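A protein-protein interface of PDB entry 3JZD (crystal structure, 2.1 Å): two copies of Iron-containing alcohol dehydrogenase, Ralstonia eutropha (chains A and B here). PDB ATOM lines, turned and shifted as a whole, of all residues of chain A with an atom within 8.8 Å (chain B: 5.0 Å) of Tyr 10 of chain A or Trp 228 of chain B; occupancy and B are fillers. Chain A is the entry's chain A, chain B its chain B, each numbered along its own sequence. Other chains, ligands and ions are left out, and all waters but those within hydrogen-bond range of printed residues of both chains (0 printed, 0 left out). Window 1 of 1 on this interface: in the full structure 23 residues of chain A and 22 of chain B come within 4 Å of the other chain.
The backbone NH (N) of Phe 19 of chain B sits at hydrogen-bond distance from the backbone carbonyl oxygen (O) of Phe 8 of chain A. The backbone NH (N) of Tyr 10 of chain A is in hydrogen-bond range of the backbone carbonyl oxygen (O) of Val 17 of chain B, at 2.8 Å. The side-chain carboxylate (OE2) of Glu 11 of chain A is in salt-bridge range of the guanidinium group (NH1) of Arg 16 of chain B (3.0 Å). N of Ala 12 of chain A is in hydrogen-bond range of O of Ala 15 of chain B (3.1 Å).
The backbone NH (N) of Val 191 of chain A lies within hydrogen-bond range of the side-chain amide oxygen (OD1) of Asn 189 of chain A, at 3.0 Å. The backbone carbonyl oxygen (O) of Trp 228 of chain B is in hydrogen-bond range of the side-chain hydroxyl (OG1) of Thr 232 of chain B, 2.9 Å away.
Among the printed residues, pairs that only touch across the chains: Pro 7 of chain A with Phe 19 of chain B (3.2 Å), Phe 8 of chain A with Val 17 of chain B (3.9 Å), Phe 8 of chain A with Trp 228 of chain B (3.8 Å), Ile 9 of chain A with Arg 16 of chain B (3.7 Å), Ile 9 of chain A with Val 17 of chain B (3.3 Å), Tyr 10 of chain A with Ala 15 of chain B (3.8 Å), Tyr 10 of chain A with Arg 16 of chain B (3.5 Å), Tyr 10 of chain A with Trp 228 of chain B (3.5 Å), Glu 11 of chain A with Ala 15 of chain B (3.2 Å), Pro 190 of chain A with Tyr 225 of chain B (3.3 Å), Val 191 of chain A with Tyr 225 of chain B (3.98 Å) and Val 191 of chain A with Trp 228 of chain B (3.4 Å).
Tyr 10 of chain A touches just these residues of chain B: Ala 15 (3.8 Å), Arg 16 (3.5 Å), Val 17 (2.8 Å) and Trp 228 (3.5 Å). Trp 228 of chain B touches three residues of chain A. Val 17 of chain B touches just these residues of chain A: Phe 8 (3.9 Å), Ile 9 (3.3 Å) and Tyr 10 (2.8 Å). No residue of chain A comes within 4 Å of Ala 227 of chain B. Of the printed residues of chain B, Glu 11 of chain A touches Ala 15 and Arg 16. Of the printed residues of chain A, Arg 16 of chain B touches Ile 9 (3.7 Å), Tyr 10 (3.5 Å) and Glu 11 (3.0 Å). Printed residues of chain A within 4 Å of Phe 19 of chain B: Pro 7 (3.2 Å) and Phe 8 (2.9 Å). Printed residues of chain B within 4 Å of Pro 7 of chain A: Phe 19 (3.2 Å). Of the printed residues of chain B, Ala 12 of chain A touches Ala 15 (3.1 Å). Leu 229 of chain B touches none of the printed residues of chain A. The nearest printed residue of chain B that does not touch Tyr 10 of chain A is Phe 19 of chain B (5.8 Å). The nearest residue of chain A that does not touch Trp 228 of chain B is Asn 189 of chain A (5.7 Å).
Of the 18 printed residues of chain A, 8 touch a printed residue of chain B. Hydrophobic or aromatic side chains of chain B within 4 Å of the printed part of chain A: Phe 19, Tyr 225 and Trp 228. Among the printed residues, Asp or Glu carboxylates within 4 Å of a Lys or Arg side-chain nitrogen of the other chain: Glu 11 of chain A with Arg 16 of chain B (3.0 Å).
2 positions are printed for both chains.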
ATOM      1  N   PRO A   7     -26.354  14.429  22.275  1.00  0.00           N
ATOM      2  CA  PRO A   7     -25.801  13.858  21.048  1.00  0.00           C
ATOM      3  C   PRO A   7     -26.061  14.739  19.809  1.00  0.00           C
ATOM      4  O   PRO A   7     -26.974  15.544  19.831  1.00  0.00           O
ATOM      5  CB  PRO A   7     -26.541  12.531  20.925  1.00  0.00           C
ATOM      6  CG  PRO A   7     -27.806  12.773  21.546  1.00  0.00           C
ATOM      7  CD  PRO A   7     -27.570  13.717  22.693  1.00  0.00           C
ATOM      8  N   PHE A   8     -25.267  14.588  18.744  1.00  0.00           N
ATOM      9  CA  PHE A   8     -25.458  15.399  17.557  1.00  0.00           C
ATOM     10  C   PHE A   8     -24.782  14.764  16.361  1.00  0.00           C
ATOM     11  O   PHE A   8     -23.985  13.860  16.521  1.00  0.00           O
ATOM     12  CB  PHE A   8     -24.897  16.832  17.777  1.00  0.00           C
ATOM     13  CG  PHE A   8     -23.417  16.851  18.144  1.00  0.00           C
ATOM     14  CD1 PHE A   8     -22.451  16.853  17.170  1.00  0.00           C
ATOM     15  CD2 PHE A   8     -23.015  16.822  19.478  1.00  0.00           C
ATOM     16  CE1 PHE A   8     -21.100  16.854  17.498  1.00  0.00           C
ATOM     17  CE2 PHE A   8     -21.689  16.825  19.822  1.00  0.00           C
ATOM     18  CZ  PHE A   8     -20.719  16.823  18.828  1.00  0.00           C
ATOM     19  N   ILE A   9     -25.140  15.241  15.172  1.00  0.00           N
ATOM     20  CA  ILE A   9     -24.504  14.842  13.943  1.00  0.00           C
ATOM     21  C   ILE A   9     -23.977  16.108  13.303  1.00  0.00           C
ATOM     22  O   ILE A   9     -24.737  17.025  13.013  1.00  0.00           O
ATOM     23  CB  ILE A   9     -25.421  14.097  12.971  1.00  0.00           C
ATOM     24  CG1 ILE A   9     -25.809  12.744  13.585  1.00  0.00           C
ATOM     25  CG2 ILE A   9     -24.685  13.877  11.638  1.00  0.00           C
ATOM     26  CD1 ILE A   9     -26.762  11.883  12.756  1.00  0.00           C
ATOM     27  N   TYR A  10     -22.663  16.166  13.114  1.00  0.00           N
ATOM     28  CA  TYR A  10     -22.028  17.298  12.534  1.00  0.00           C
ATOM     29  C   TYR A  10     -21.683  16.945  11.126  1.00  0.00           C
ATOM     30  O   TYR A  10     -21.136  15.879  10.853  1.00  0.00           O
ATOM     31  CB  TYR A  10     -20.741  17.648  13.287  1.00  0.00           C
ATOM     32  CG  TYR A  10     -19.851  18.656  12.582  1.00  0.00           C
ATOM     33  CD1 TYR A  10     -20.011  20.013  12.786  1.00  0.00           C
ATOM     34  CD2 TYR A  10     -18.839  18.247  11.719  1.00  0.00           C
ATOM     35  CE1 TYR A  10     -19.211  20.910  12.170  1.00  0.00           C
ATOM     36  CE2 TYR A  10     -18.033  19.160  11.107  1.00  0.00           C
ATOM     37  CZ  TYR A  10     -18.223  20.478  11.336  1.00  0.00           C
ATOM     38  OH  TYR A  10     -17.429  21.392  10.741  1.00  0.00           O
ATOM     39  N   GLU A  11     -21.966  17.880  10.244  1.00  0.00           N
ATOM     40  CA  GLU A  11     -21.601  17.736   8.860  1.00  0.00           C
ATOM     41  C   GLU A  11     -20.921  19.007   8.400  1.00  0.00           C
ATOM     42  O   GLU A  11     -21.370  20.152   8.695  1.00  0.00           O
ATOM     43  CB  GLU A  11     -22.808  17.411   8.002  1.00  0.00           C
ATOM     44  CG  GLU A  11     -23.141  15.949   8.062  1.00  0.00           C
ATOM     45  CD  GLU A  11     -24.345  15.553   7.229  1.00  0.00           C
ATOM     46  OE1 GLU A  11     -25.374  16.300   7.301  1.00  0.00           O
ATOM     47  OE2 GLU A  11     -24.252  14.466   6.558  1.00  0.00           O
ATOM     48  N   ALA A  12     -19.798  18.823   7.735  1.00  0.00           N
ATOM     49  CA  ALA A  12     -19.134  19.960   7.167  1.00  0.00           C
ATOM     50  C   ALA A  12     -19.229  19.779   5.663  1.00  0.00           C
ATOM     51  O   ALA A  12     -19.023  18.680   5.135  1.00  0.00           O
ATOM     52  CB  ALA A  12     -17.694  20.028   7.621  1.00  0.00           C
ATOM     53  N   HIS A  13     -19.569  20.868   4.985  1.00  0.00           N
ATOM     54  CA  HIS A  13     -19.545  20.911   3.532  1.00  0.00           C
ATOM     55  C   HIS A  13     -18.067  21.028   3.086  1.00  0.00           C
ATOM     56  O   HIS A  13     -17.287  21.627   3.800  1.00  0.00           O
ATOM     57  CB  HIS A  13     -20.265  22.179   3.044  1.00  0.00           C
ATOM     58  CG  HIS A  13     -21.720  22.274   3.406  1.00  0.00           C
ATOM     59  ND1 HIS A  13     -22.669  21.380   2.950  1.00  0.00           N
ATOM     60  CD2 HIS A  13     -22.403  23.216   4.103  1.00  0.00           C
ATOM     61  CE1 HIS A  13     -23.860  21.741   3.392  1.00  0.00           C
ATOM     62  NE2 HIS A  13     -23.726  22.845   4.107  1.00  0.00           N
ATOM     63  N   ASP A 187     -31.179  21.650  15.757  1.00  0.00           N
ATOM     64  CA  ASP A 187     -30.049  20.758  15.424  1.00  0.00           C
ATOM     65  C   ASP A 187     -28.693  21.417  15.700  1.00  0.00           C
ATOM     66  O   ASP A 187     -27.676  21.155  15.041  1.00  0.00           O
ATOM     67  CB  ASP A 187     -30.154  20.261  13.969  1.00  0.00           C
ATOM     68  CG  ASP A 187     -30.191  21.392  12.943  1.00  0.00           C
ATOM     69  OD1 ASP A 187     -30.504  22.557  13.304  1.00  0.00           O
ATOM     70  OD2 ASP A 187     -29.907  21.101  11.760  1.00  0.00           O
ATOM     71  N   ALA A 188     -28.696  22.268  16.713  1.00  0.00           N
ATOM     72  CA  ALA A 188     -27.507  22.918  17.181  1.00  0.00           C
ATOM     73  C   ALA A 188     -26.455  21.879  17.499  1.00  0.00           C
ATOM     74  O   ALA A 188     -26.785  20.773  17.938  1.00  0.00           O
ATOM     75  CB  ALA A 188     -27.831  23.707  18.456  1.00  0.00           C
ATOM     76  N   ASN A 189     -25.193  22.192  17.208  1.00  0.00           N
ATOM     77  CA  ASN A 189     -24.101  21.348  17.674  1.00  0.00           C
ATOM     78  C   ASN A 189     -22.930  22.240  18.177  1.00  0.00           C
ATOM     79  O   ASN A 189     -22.852  23.441  17.839  1.00  0.00           O
ATOM     80  CB  ASN A 189     -23.695  20.317  16.619  1.00  0.00           C
ATOM     81  CG  ASN A 189     -22.942  20.916  15.484  1.00  0.00           C
ATOM     82  OD1 ASN A 189     -21.870  21.485  15.684  1.00  0.00           O
ATOM     83  ND2 ASN A 189     -23.480  20.780  14.267  1.00  0.00           N
ATOM     84  N   PRO A 190     -22.010  21.656  18.992  1.00  0.00           N
ATOM     85  CA  PRO A 190     -20.924  22.435  19.625  1.00  0.00           C
ATOM     86  C   PRO A 190     -19.973  23.129  18.685  1.00  0.00           C
ATOM     87  O   PRO A 190     -19.416  24.189  19.011  1.00  0.00           O
ATOM     88  CB  PRO A 190     -20.186  21.395  20.471  1.00  0.00           C
ATOM     89  CG  PRO A 190     -21.202  20.288  20.674  1.00  0.00           C
ATOM     90  CD  PRO A 190     -22.081  20.274  19.484  1.00  0.00           C
ATOM     91  N   VAL A 191     -19.757  22.539  17.516  1.00  0.00           N
ATOM     92  CA  VAL A 191     -18.828  23.130  16.578  1.00  0.00           C
ATOM     93  C   VAL A 191     -19.487  24.323  15.902  1.00  0.00           C
ATOM     94  O   VAL A 191     -18.917  25.401  15.811  1.00  0.00           O
ATOM     95  CB  VAL A 191     -18.287  22.081  15.601  1.00  0.00           C
ATOM     96  CG1 VAL A 191     -17.441  22.734  14.619  1.00  0.00           C
ATOM     97  CG2 VAL A 191     -17.479  20.989  16.411  1.00  0.00           C
ATOM     98  N   MET A 192     -20.719  24.148  15.459  1.00  0.00           N
ATOM     99  CA  MET A 192     -21.466  25.250  14.870  1.00  0.00           C
ATOM    100  C   MET A 192     -21.632  26.391  15.920  1.00  0.00           C
ATOM    101  O   MET A 192     -21.498  27.591  15.602  1.00  0.00           O
ATOM    102  CB  MET A 192     -22.806  24.745  14.343  1.00  0.00           C
ATOM    103  CG  MET A 192     -22.666  23.874  13.117  1.00  0.00           C
ATOM    104  SD  MET A 192     -22.168  24.944  11.557  1.00  0.00           S
ATOM    105  CE  MET A 192     -21.078  23.631  10.613  1.00  0.00           C
ATOM    106  N   SER A 193     -21.893  26.019  17.160  1.00  0.00           N
ATOM    107  CA  SER A 193     -22.041  27.013  18.205  1.00  0.00           C
ATOM    108  C   SER A 193     -20.763  27.771  18.515  1.00  0.00           C
ATOM    109  O   SER A 193     -20.817  28.968  18.785  1.00  0.00           O
ATOM    110  CB  SER A 193     -22.610  26.354  19.460  1.00  0.00           C
ATOM    111  OG  SER A 193     -23.930  25.958  19.137  1.00  0.00           O
ATOM    112  N   MET A 195     -18.440  28.387  16.291  1.00  0.00           N
ATOM    113  CA  MET A 195     -18.227  29.325  15.214  1.00  0.00           C
ATOM    114  C   MET A 195     -19.269  30.457  15.307  1.00  0.00           C
ATOM    115  O   MET A 195     -18.946  31.618  14.986  1.00  0.00           O
ATOM    116  CB  MET A 195     -18.267  28.624  13.859  1.00  0.00           C
ATOM    117  CG  MET A 195     -17.253  27.480  13.735  1.00  0.00           C
ATOM    118  SD  MET A 195     -17.399  26.711  11.955  1.00  0.00           S
ATOM    119  CE  MET A 195     -16.680  28.173  10.981  1.00  0.00           C
ATOM    120  N   THR A 232     -21.513  30.046   7.667  1.00  0.00           N
ATOM    121  CA  THR A 232     -21.259  28.632   7.850  1.00  0.00           C
ATOM    122  C   THR A 232     -22.308  28.085   8.806  1.00  0.00           C
ATOM    123  O   THR A 232     -22.825  26.996   8.564  1.00  0.00           O
ATOM    124  CB  THR A 232     -19.847  28.351   8.354  1.00  0.00           C
ATOM    125  OG1 THR A 232     -18.906  28.956   7.451  1.00  0.00           O
ATOM    126  CG2 THR A 232     -19.621  26.858   8.461  1.00  0.00           C
ATOM    127  N   GLY A 236     -25.327  25.192   8.031  1.00  0.00           N
ATOM    128  CA  GLY A 236     -25.235  23.937   8.746  1.00  0.00           C
ATOM    129  C   GLY A 236     -26.307  23.580   9.763  1.00  0.00           C
ATOM    130  O   GLY A 236     -26.449  22.412  10.067  1.00  0.00           O
ATOM    131  N   VAL A 237     -27.054  24.541  10.291  1.00  0.00           N
ATOM    132  CA  VAL A 237     -28.123  24.249  11.257  1.00  0.00           C
ATOM    133  C   VAL A 237     -29.374  25.026  10.877  1.00  0.00           C
ATOM    134  O   VAL A 237     -29.305  25.935  10.044  1.00  0.00           O
ATOM    135  CB  VAL A 237     -27.679  24.546  12.728  1.00  0.00           C
ATOM    136  CG1 VAL A 237     -26.385  23.768  13.066  1.00  0.00           C
ATOM    137  CG2 VAL A 237     -27.463  26.023  12.952  1.00  0.00           C
ATOM    138  N   ALA B  15     -17.265  16.220   5.797  1.00  0.00           N
ATOM    139  CA  ALA B  15     -17.166  15.379   7.005  1.00  0.00           C
ATOM    140  C   ALA B  15     -18.534  15.015   7.527  1.00  0.00           C
ATOM    141  O   ALA B  15     -19.469  15.805   7.393  1.00  0.00           O
ATOM    142  CB  ALA B  15     -16.412  16.128   8.092  1.00  0.00           C
ATOM    143  N   ARG B  16     -18.643  13.810   8.095  1.00  0.00           N
ATOM    144  CA  ARG B  16     -19.828  13.387   8.810  1.00  0.00           C
ATOM    145  C   ARG B  16     -19.380  12.739  10.132  1.00  0.00           C
ATOM    146  O   ARG B  16     -18.663  11.736  10.123  1.00  0.00           O
ATOM    147  CB  ARG B  16     -20.641  12.416   7.994  1.00  0.00           C
ATOM    148  CG  ARG B  16     -21.913  12.000   8.726  1.00  0.00           C
ATOM    149  CD  ARG B  16     -22.785  11.143   7.817  1.00  0.00           C
ATOM    150  NE  ARG B  16     -23.889  10.555   8.569  1.00  0.00           N
ATOM    151  CZ  ARG B  16     -25.070  11.128   8.768  1.00  0.00           C
ATOM    152  NH1 ARG B  16     -25.353  12.316   8.268  1.00  0.00           N
ATOM    153  NH2 ARG B  16     -25.984  10.479   9.462  1.00  0.00           N
ATOM    154  N   VAL B  17     -19.832  13.298  11.251  1.00  0.00           N
ATOM    155  CA  VAL B  17     -19.445  12.883  12.577  1.00  0.00           C
ATOM    156  C   VAL B  17     -20.696  12.723  13.420  1.00  0.00           C
ATOM    157  O   VAL B  17     -21.452  13.678  13.607  1.00  0.00           O
ATOM    158  CB  VAL B  17     -18.533  13.977  13.247  1.00  0.00           C
ATOM    159  CG1 VAL B  17     -18.142  13.591  14.663  1.00  0.00           C
ATOM    160  CG2 VAL B  17     -17.286  14.241  12.391  1.00  0.00           C
ATOM    161  N   PHE B  19     -21.925  11.910  17.024  1.00  0.00           N
ATOM    162  CA  PHE B  19     -21.328  12.047  18.311  1.00  0.00           C
ATOM    163  C   PHE B  19     -22.316  11.873  19.448  1.00  0.00           C
ATOM    164  O   PHE B  19     -23.426  12.419  19.443  1.00  0.00           O
ATOM    165  CB  PHE B  19     -20.647  13.426  18.404  1.00  0.00           C
ATOM    166  CG  PHE B  19     -19.774  13.583  19.608  1.00  0.00           C
ATOM    167  CD1 PHE B  19     -20.338  13.750  20.874  1.00  0.00           C
ATOM    168  CD2 PHE B  19     -18.389  13.497  19.494  1.00  0.00           C
ATOM    169  CE1 PHE B  19     -19.520  13.856  22.005  1.00  0.00           C
ATOM    170  CE2 PHE B  19     -17.571  13.602  20.620  1.00  0.00           C
ATOM    171  CZ  PHE B  19     -18.139  13.793  21.868  1.00  0.00           C
ATOM    172  N   GLU B 127      -8.460   9.538  12.819  1.00  0.00           N
ATOM    173  CA  GLU B 127      -9.722   9.440  12.095  1.00  0.00           C
ATOM    174  C   GLU B 127     -10.103  10.643  11.226  1.00  0.00           C
ATOM    175  O   GLU B 127     -10.944  10.521  10.334  1.00  0.00           O
ATOM    176  CB  GLU B 127     -10.881   9.132  13.057  1.00  0.00           C
ATOM    177  CG  GLU B 127     -11.144  10.144  14.146  1.00  0.00           C
ATOM    178  CD  GLU B 127     -10.281   9.979  15.412  1.00  0.00           C
ATOM    179  OE1 GLU B 127      -9.241   9.304  15.402  1.00  0.00           O
ATOM    180  OE2 GLU B 127     -10.636  10.604  16.406  1.00  0.00           O
ATOM    181  N   VAL B 128      -9.533  11.806  11.516  1.00  0.00           N
ATOM    182  CA  VAL B 128      -9.812  12.973  10.724  1.00  0.00           C
ATOM    183  C   VAL B 128      -8.564  13.562  10.041  1.00  0.00           C
ATOM    184  O   VAL B 128      -8.510  14.773   9.785  1.00  0.00           O
ATOM    185  CB  VAL B 128     -10.544  14.023  11.557  1.00  0.00           C
ATOM    186  CG1 VAL B 128     -11.958  13.557  11.816  1.00  0.00           C
ATOM    187  CG2 VAL B 128      -9.803  14.287  12.854  1.00  0.00           C
ATOM    188  N   TYR B 155     -18.303   8.728  17.159  1.00  0.00           N
ATOM    189  CA  TYR B 155     -17.691   8.942  18.474  1.00  0.00           C
ATOM    190  C   TYR B 155     -18.645   8.514  19.551  1.00  0.00           C
ATOM    191  O   TYR B 155     -19.667   9.189  19.778  1.00  0.00           O
ATOM    192  CB  TYR B 155     -17.313  10.409  18.700  1.00  0.00           C
ATOM    193  CG  TYR B 155     -16.104  10.894  17.923  1.00  0.00           C
ATOM    194  CD1 TYR B 155     -14.856  10.326  18.139  1.00  0.00           C
ATOM    195  CD2 TYR B 155     -16.190  11.943  17.023  1.00  0.00           C
ATOM    196  CE1 TYR B 155     -13.741  10.748  17.458  1.00  0.00           C
ATOM    197  CE2 TYR B 155     -15.065  12.399  16.340  1.00  0.00           C
ATOM    198  CZ  TYR B 155     -13.841  11.785  16.561  1.00  0.00           C
ATOM    199  OH  TYR B 155     -12.703  12.191  15.912  1.00  0.00           O
ATOM    200  N   MET B 195     -10.600  26.035  16.813  1.00  0.00           N
ATOM    201  CA  MET B 195     -10.806  24.637  17.196  1.00  0.00           C
ATOM    202  C   MET B 195      -9.671  24.114  18.072  1.00  0.00           C
ATOM    203  O   MET B 195      -9.919  23.360  19.005  1.00  0.00           O
ATOM    204  CB  MET B 195     -10.946  23.745  15.971  1.00  0.00           C
ATOM    205  CG  MET B 195     -12.138  24.100  15.163  1.00  0.00           C
ATOM    206  SD  MET B 195     -12.369  22.983  13.639  1.00  0.00           S
ATOM    207  CE  MET B 195     -12.343  21.265  14.497  1.00  0.00           C
ATOM    208  N   LEU B 224     -13.198  13.008  24.097  1.00  0.00           N
ATOM    209  CA  LEU B 224     -13.391  12.590  22.727  1.00  0.00           C
ATOM    210  C   LEU B 224     -13.699  13.792  21.844  1.00  0.00           C
ATOM    211  O   LEU B 224     -13.260  13.828  20.724  1.00  0.00           O
ATOM    212  CB  LEU B 224     -14.490  11.550  22.684  1.00  0.00           C
ATOM    213  CG  LEU B 224     -14.464  10.439  21.660  1.00  0.00           C
ATOM    214  CD1 LEU B 224     -13.093   9.757  21.570  1.00  0.00           C
ATOM    215  CD2 LEU B 224     -15.572   9.401  22.007  1.00  0.00           C
ATOM    216  N   TYR B 225     -14.470  14.750  22.366  1.00  0.00           N
ATOM    217  CA  TYR B 225     -14.765  15.961  21.662  1.00  0.00           C
ATOM    218  C   TYR B 225     -13.467  16.725  21.410  1.00  0.00           C
ATOM    219  O   TYR B 225     -13.204  17.197  20.294  1.00  0.00           O
ATOM    220  CB  TYR B 225     -15.728  16.821  22.475  1.00  0.00           C
ATOM    221  CG  TYR B 225     -16.005  18.183  21.879  1.00  0.00           C
ATOM    222  CD1 TYR B 225     -16.631  18.299  20.652  1.00  0.00           C
ATOM    223  CD2 TYR B 225     -15.705  19.360  22.579  1.00  0.00           C
ATOM    224  CE1 TYR B 225     -16.916  19.539  20.104  1.00  0.00           C
ATOM    225  CE2 TYR B 225     -16.004  20.616  22.043  1.00  0.00           C
ATOM    226  CZ  TYR B 225     -16.589  20.685  20.793  1.00  0.00           C
ATOM    227  OH  TYR B 225     -16.924  21.894  20.244  1.00  0.00           O
ATOM    228  N   GLY B 226     -12.672  16.857  22.459  1.00  0.00           N
ATOM    229  CA  GLY B 226     -11.365  17.492  22.332  1.00  0.00           C
ATOM    230  C   GLY B 226     -10.487  16.782  21.321  1.00  0.00           C
ATOM    231  O   GLY B 226      -9.839  17.444  20.491  1.00  0.00           O
ATOM    232  N   ALA B 227     -10.474  15.440  21.370  1.00  0.00           N
ATOM    233  CA  ALA B 227      -9.649  14.626  20.458  1.00  0.00           C
ATOM    234  C   ALA B 227     -10.009  14.930  18.984  1.00  0.00           C
ATOM    235  O   ALA B 227      -9.128  14.991  18.123  1.00  0.00           O
ATOM    236  CB  ALA B 227      -9.801  13.096  20.724  1.00  0.00           C
ATOM    237  N   TRP B 228     -11.303  15.080  18.720  1.00  0.00           N
ATOM    238  CA  TRP B 228     -11.805  15.335  17.380  1.00  0.00           C
ATOM    239  C   TRP B 228     -11.315  16.692  16.896  1.00  0.00           C
ATOM    240  O   TRP B 228     -10.759  16.816  15.798  1.00  0.00           O
ATOM    241  CB  TRP B 228     -13.346  15.221  17.388  1.00  0.00           C
ATOM    242  CG  TRP B 228     -14.028  15.755  16.185  1.00  0.00           C
ATOM    243  CD1 TRP B 228     -13.615  15.651  14.882  1.00  0.00           C
ATOM    244  CD2 TRP B 228     -15.288  16.392  16.152  1.00  0.00           C
ATOM    245  NE1 TRP B 228     -14.498  16.272  14.068  1.00  0.00           N
ATOM    246  CE2 TRP B 228     -15.548  16.730  14.814  1.00  0.00           C
ATOM    247  CE3 TRP B 228     -16.224  16.739  17.129  1.00  0.00           C
ATOM    248  CZ2 TRP B 228     -16.729  17.371  14.417  1.00  0.00           C
ATOM    249  CZ3 TRP B 228     -17.386  17.399  16.740  1.00  0.00           C
ATOM    250  CH2 TRP B 228     -17.627  17.707  15.395  1.00  0.00           C
ATOM    251  N   LEU B 229     -11.486  17.703  17.726  1.00  0.00           N
ATOM    252  CA  LEU B 229     -11.016  19.054  17.356  1.00  0.00           C
ATOM    253  C   LEU B 229      -9.488  19.083  17.083  1.00  0.00           C
ATOM    254  O   LEU B 229      -9.020  19.672  16.102  1.00  0.00           O
ATOM    255  CB  LEU B 229     -11.419  20.092  18.430  1.00  0.00           C
ATOM    256  CG  LEU B 229     -12.923  20.388  18.589  1.00  0.00           C
ATOM    257  CD1 LEU B 229     -13.159  21.565  19.474  1.00  0.00           C
ATOM    258  CD2 LEU B 229     -13.585  20.589  17.267  1.00  0.00           C
ATOM    259  N   CYS B 230      -8.723  18.420  17.962  1.00  0.00           N
ATOM    260  CA  CYS B 230      -7.258  18.399  17.846  1.00  0.00           C
ATOM    261  C   CYS B 230      -6.864  17.632  16.619  1.00  0.00           C
ATOM    262  O   CYS B 230      -5.911  18.010  15.940  1.00  0.00           O
ATOM    263  CB  CYS B 230      -6.609  17.812  19.074  1.00  0.00           C
ATOM    264  SG  CYS B 230      -6.872  18.734  20.600  1.00  0.00           S
ATOM    265  N   GLY B 231      -7.608  16.574  16.323  1.00  0.00           N
ATOM    266  CA  GLY B 231      -7.353  15.772  15.131  1.00  0.00           C
ATOM    267  C   GLY B 231      -7.623  16.557  13.862  1.00  0.00           C
ATOM    268  O   GLY B 231      -6.885  16.442  12.867  1.00  0.00           O
ATOM    269  N   THR B 232      -8.687  17.351  13.890  1.00  0.00           N
ATOM    270  CA  THR B 232      -9.043  18.208  12.782  1.00  0.00           C
ATOM    271  C   THR B 232      -7.923  19.231  12.501  1.00  0.00           C
ATOM    272  O   THR B 232      -7.587  19.483  11.352  1.00  0.00           O
ATOM    273  CB  THR B 232     -10.418  18.897  13.053  1.00  0.00           C
ATOM    274  OG1 THR B 232     -11.451  17.881  13.177  1.00  0.00           O
ATOM    275  CG2 THR B 232     -10.806  19.859  11.942  1.00  0.00           C
